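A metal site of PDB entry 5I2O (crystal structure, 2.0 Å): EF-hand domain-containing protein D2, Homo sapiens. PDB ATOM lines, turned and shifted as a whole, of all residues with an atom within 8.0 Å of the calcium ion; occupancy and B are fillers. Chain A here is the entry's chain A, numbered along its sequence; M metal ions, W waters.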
ATOM      1  N   PHE A  47      15.542  14.570  23.464  1.00  0.00           N
ATOM      2  CA  PHE A  47      15.915  15.921  23.210  1.00  0.00           C
ATOM      3  C   PHE A  47      16.397  16.613  24.446  1.00  0.00           C
ATOM      4  O   PHE A  47      15.922  16.385  25.517  1.00  0.00           O
ATOM      5  CB  PHE A  47      14.747  16.692  22.639  1.00  0.00           C
ATOM      6  CG  PHE A  47      14.323  16.228  21.301  1.00  0.00           C
ATOM      7  CD1 PHE A  47      13.420  15.185  21.173  1.00  0.00           C
ATOM      8  CD2 PHE A  47      14.830  16.809  20.179  1.00  0.00           C
ATOM      9  CE1 PHE A  47      13.031  14.758  19.930  1.00  0.00           C
ATOM     10  CE2 PHE A  47      14.450  16.380  18.933  1.00  0.00           C
ATOM     11  CZ  PHE A  47      13.540  15.345  18.815  1.00  0.00           C
ATOM     12  N   ILE A  48      17.376  17.479  24.285  1.00  0.00           N
ATOM     13  CA  ILE A  48      17.821  18.299  25.398  1.00  0.00           C
ATOM     14  C   ILE A  48      17.335  19.697  25.110  1.00  0.00           C
ATOM     15  O   ILE A  48      17.803  20.340  24.179  1.00  0.00           O
ATOM     16  CB  ILE A  48      19.357  18.244  25.514  1.00  0.00           C
ATOM     17  CG1 ILE A  48      19.795  16.832  25.897  1.00  0.00           C
ATOM     18  CG2 ILE A  48      19.859  19.248  26.540  1.00  0.00           C
ATOM     19  CD1 ILE A  48      21.225  16.772  26.362  1.00  0.00           C
ATOM     20  N   ILE A  73      22.532  26.561  21.931  1.00  0.00           N
ATOM     21  CA  ILE A  73      21.589  25.777  21.112  1.00  0.00           C
ATOM     22  C   ILE A  73      21.506  26.261  19.664  1.00  0.00           C
ATOM     23  O   ILE A  73      21.589  25.463  18.714  1.00  0.00           O
ATOM     24  CB  ILE A  73      20.187  25.744  21.771  1.00  0.00           C
ATOM     25  CG1 ILE A  73      20.330  24.957  23.091  1.00  0.00           C
ATOM     26  CG2 ILE A  73      19.136  25.107  20.829  1.00  0.00           C
ATOM     27  CD1 ILE A  73      19.102  24.959  23.959  1.00  0.00           C
ATOM     28  N   VAL A  76      24.020  25.041  16.868  1.00  0.00           N
ATOM     29  CA  VAL A  76      23.864  23.714  16.249  1.00  0.00           C
ATOM     30  C   VAL A  76      22.400  23.293  15.963  1.00  0.00           C
ATOM     31  O   VAL A  76      22.160  22.137  15.569  1.00  0.00           O
ATOM     32  CB  VAL A  76      24.491  22.650  17.148  1.00  0.00           C
ATOM     33  CG1 VAL A  76      26.049  22.792  17.194  1.00  0.00           C
ATOM     34  CG2 VAL A  76      23.899  22.755  18.565  1.00  0.00           C
ATOM     35  N   ASP A  77      21.437  24.185  16.149  1.00  0.00           N
ATOM     36  CA  ASP A  77      20.024  23.769  16.099  1.00  0.00           C
ATOM     37  C   ASP A  77      19.552  23.750  14.643  1.00  0.00           C
ATOM     38  O   ASP A  77      18.829  24.649  14.184  1.00  0.00           O
ATOM     39  CB  ASP A  77      19.153  24.717  16.910  1.00  0.00           C
ATOM     40  CG  ASP A  77      17.679  24.324  16.893  1.00  0.00           C
ATOM     41  OD1 ASP A  77      17.337  23.141  16.631  1.00  0.00           O
ATOM     42  OD2 ASP A  77      16.838  25.204  17.140  1.00  0.00           O
ATOM     43  N   GLU A  78      19.956  22.699  13.911  1.00  0.00           N
ATOM     44  CA  GLU A  78      19.742  22.652  12.452  1.00  0.00           C
ATOM     45  C   GLU A  78      18.299  22.478  12.031  1.00  0.00           C
ATOM     46  O   GLU A  78      17.943  22.790  10.890  1.00  0.00           O
ATOM     47  CB  GLU A  78      20.671  21.602  11.817  1.00  0.00           C
ATOM     48  CG  GLU A  78      22.121  22.048  11.866  1.00  0.00           C
ATOM     49  CD  GLU A  78      23.060  21.247  10.953  1.00  0.00           C
ATOM     50  OE1 GLU A  78      22.767  20.063  10.684  1.00  0.00           O
ATOM     51  OE2 GLU A  78      24.114  21.809  10.540  1.00  0.00           O
ATOM     52  N   ASP A  79      17.433  22.028  12.940  1.00  0.00           N
ATOM     53  CA  ASP A  79      16.019  21.907  12.588  1.00  0.00           C
ATOM     54  C   ASP A  79      15.148  22.940  13.286  1.00  0.00           C
ATOM     55  O   ASP A  79      13.906  22.847  13.283  1.00  0.00           O
ATOM     56  CB  ASP A  79      15.493  20.494  12.825  1.00  0.00           C
ATOM     57  CG  ASP A  79      15.585  20.066  14.274  1.00  0.00           C
ATOM     58  OD1 ASP A  79      15.898  20.908  15.147  1.00  0.00           O
ATOM     59  OD2 ASP A  79      15.325  18.882  14.533  1.00  0.00           O
ATOM     60  N   PHE A  80      15.803  23.928  13.919  1.00  0.00           N
ATOM     61  CA  PHE A  80      15.119  25.126  14.415  1.00  0.00           C
ATOM     62  C   PHE A  80      13.938  24.848  15.344  1.00  0.00           C
ATOM     63  O   PHE A  80      12.879  25.485  15.206  1.00  0.00           O
ATOM     64  CB  PHE A  80      14.636  25.981  13.228  1.00  0.00           C
ATOM     65  CG  PHE A  80      15.736  26.351  12.261  1.00  0.00           C
ATOM     66  CD1 PHE A  80      16.089  25.481  11.229  1.00  0.00           C
ATOM     67  CD2 PHE A  80      16.446  27.547  12.402  1.00  0.00           C
ATOM     68  CE1 PHE A  80      17.123  25.811  10.346  1.00  0.00           C
ATOM     69  CE2 PHE A  80      17.468  27.865  11.521  1.00  0.00           C
ATOM     70  CZ  PHE A  80      17.802  26.998  10.495  1.00  0.00           C
ATOM     71  N   ASP A  81      14.086  23.904  16.271  1.00  0.00           N
ATOM     72  CA  ASP A  81      12.989  23.663  17.214  1.00  0.00           C
ATOM     73  C   ASP A  81      13.421  24.061  18.612  1.00  0.00           C
ATOM     74  O   ASP A  81      12.747  23.744  19.597  1.00  0.00           O
ATOM     75  CB  ASP A  81      12.535  22.203  17.184  1.00  0.00           C
ATOM     76  CG  ASP A  81      13.608  21.234  17.581  1.00  0.00           C
ATOM     77  OD1 ASP A  81      14.778  21.652  17.843  1.00  0.00           O
ATOM     78  OD2 ASP A  81      13.319  20.020  17.619  1.00  0.00           O
ATOM     79  N   SER A  82      14.570  24.727  18.671  1.00  0.00           N
ATOM     80  CA  SER A  82      15.100  25.289  19.924  1.00  0.00           C
ATOM     81  C   SER A  82      15.438  24.207  20.958  1.00  0.00           C
ATOM     82  O   SER A  82      15.525  24.468  22.163  1.00  0.00           O
ATOM     83  CB  SER A  82      14.136  26.310  20.530  1.00  0.00           C
ATOM     84  OG  SER A  82      14.018  27.456  19.701  1.00  0.00           O
ATOM     85  N   LYS A  83      15.772  23.009  20.564  1.00  0.00           N
ATOM     86  CA  LYS A  83      16.211  21.939  21.436  1.00  0.00           C
ATOM     87  C   LYS A  83      17.163  21.064  20.678  1.00  0.00           C
ATOM     88  O   LYS A  83      17.297  21.204  19.466  1.00  0.00           O
ATOM     89  CB  LYS A  83      15.034  21.139  21.990  1.00  0.00           C
ATOM     90  CG  LYS A  83      14.170  20.422  20.938  1.00  0.00           C
ATOM     91  CD  LYS A  83      13.047  19.677  21.679  1.00  0.00           C
ATOM     92  CE  LYS A  83      12.154  18.944  20.715  1.00  0.00           C
ATOM     93  NZ  LYS A  83      11.446  19.956  19.860  1.00  0.00           N
ATOM     94  N   LEU A  84      17.908  20.319  21.374  1.00  0.00           N
ATOM     95  CA  LEU A  84      19.019  19.582  20.791  1.00  0.00           C
ATOM     96  C   LEU A  84      18.654  18.116  20.639  1.00  0.00           C
ATOM     97  O   LEU A  84      18.385  17.447  21.650  1.00  0.00           O
ATOM     98  CB  LEU A  84      20.235  19.712  21.710  1.00  0.00           C
ATOM     99  CG  LEU A  84      20.871  21.056  21.946  1.00  0.00           C
ATOM    100  CD1 LEU A  84      22.017  20.838  22.958  1.00  0.00           C
ATOM    101  CD2 LEU A  84      21.447  21.569  20.638  1.00  0.00           C
ATOM    102  N   SER A  85      18.625  17.616  19.405  1.00  0.00           N
ATOM    103  CA  SER A  85      18.568  16.172  19.179  1.00  0.00           C
ATOM    104  C   SER A  85      19.951  15.604  19.410  1.00  0.00           C
ATOM    105  O   SER A  85      20.928  16.363  19.546  1.00  0.00           O
ATOM    106  CB  SER A  85      18.171  15.854  17.745  1.00  0.00           C
ATOM    107  OG  SER A  85      19.155  16.372  16.878  1.00  0.00           O
ATOM    108  N   PHE A  86      20.066  14.282  19.442  1.00  0.00           N
ATOM    109  CA  PHE A  86      21.373  13.684  19.575  1.00  0.00           C
ATOM    110  C   PHE A  86      22.289  14.077  18.406  1.00  0.00           C
ATOM    111  O   PHE A  86      23.488  14.319  18.576  1.00  0.00           O
ATOM    112  CB  PHE A  86      21.238  12.165  19.693  1.00  0.00           C
ATOM    113  CG  PHE A  86      22.544  11.473  19.873  1.00  0.00           C
ATOM    114  CD1 PHE A  86      23.417  11.909  20.857  1.00  0.00           C
ATOM    115  CD2 PHE A  86      22.929  10.433  19.037  1.00  0.00           C
ATOM    116  CE1 PHE A  86      24.647  11.302  21.020  1.00  0.00           C
ATOM    117  CE2 PHE A  86      24.160   9.811  19.214  1.00  0.00           C
ATOM    118  CZ  PHE A  86      25.014  10.250  20.203  1.00  0.00           C
ATOM    119  N   GLU A  88      22.368  16.791  16.764  1.00  0.00           N
ATOM    120  CA  GLU A  88      22.862  18.151  16.976  1.00  0.00           C
ATOM    121  C   GLU A  88      23.870  18.206  18.122  1.00  0.00           C
ATOM    122  O   GLU A  88      24.822  18.998  18.091  1.00  0.00           O
ATOM    123  CB  GLU A  88      21.686  19.106  17.228  1.00  0.00           C
ATOM    124  CG  GLU A  88      20.771  19.222  16.019  1.00  0.00           C
ATOM    125  CD  GLU A  88      19.465  19.883  16.383  1.00  0.00           C
ATOM    126  OE1 GLU A  88      19.132  19.961  17.590  1.00  0.00           O
ATOM    127  OE2 GLU A  88      18.762  20.336  15.453  1.00  0.00           O
ATOM    128  N   PHE A  89      23.679  17.367  19.131  1.00  0.00           N
ATOM    129  CA  PHE A  89      24.674  17.224  20.198  1.00  0.00           C
ATOM    130  C   PHE A  89      26.021  16.800  19.598  1.00  0.00           C
ATOM    131  O   PHE A  89      27.089  17.350  19.941  1.00  0.00           O
ATOM    132  CB  PHE A  89      24.185  16.203  21.226  1.00  0.00           C
ATOM    133  CG  PHE A  89      24.972  16.215  22.501  1.00  0.00           C
ATOM    134  CD1 PHE A  89      24.924  17.323  23.368  1.00  0.00           C
ATOM    135  CD2 PHE A  89      25.768  15.118  22.855  1.00  0.00           C
ATOM    136  CE1 PHE A  89      25.667  17.350  24.561  1.00  0.00           C
ATOM    137  CE2 PHE A  89      26.509  15.131  24.047  1.00  0.00           C
ATOM    138  CZ  PHE A  89      26.478  16.258  24.888  1.00  0.00           C
HETATM  139 CA    CA M   1      16.972  20.971  17.211  1.00  0.00          CA
HETATM  140  O   HOH W   1      15.946  18.837  17.396  1.00  0.00           O
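Water W1 lies within hydrogen-bond range of the side-chain carboxylate (OD2) of Asp 81 (2.9 Å) and the side-chain carboxylate (OD2) of Asp 79 (2.9 Å).
The backbone NH (N) of Phe 80 sits close to the side-chain carboxylate (OD1) of Asp 77 (3.2 Å). The side-chain carboxylate (OE2) of Glu 88 sits close to the backbone NH (N) of Glu 78, 3.1 Å away. The side-chain carboxylate of Asp 77 lies within hydrogen-bond range of the backbone NH of Ser 82, 2.8 Å away. N of Glu 88 is in hydrogen-bond range of OG of Ser 85 (3.2 Å).
The nearest printed residue that does not touch the calcium ion is Leu 84 (4.3 Å).
The calcium ion is bound by the side-chain carboxylate (OD1) of Asp 77 (2.3 Å), the backbone carbonyl oxygen (O) of Lys 83 (2.3 Å), the side-chain carboxylate (OD1) of Asp 79 (2.3 Å), water W1 (2.4 Å), the side-chain carboxylate (OD1) of Asp 81 (2.4 Å), the side-chain carboxylate (OE1) of Glu 88 (2.4 Å) and the side-chain carboxylate (OE2) of Glu 88 (2.6 Å). The calcium ion has seven donor atoms within binding distance.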
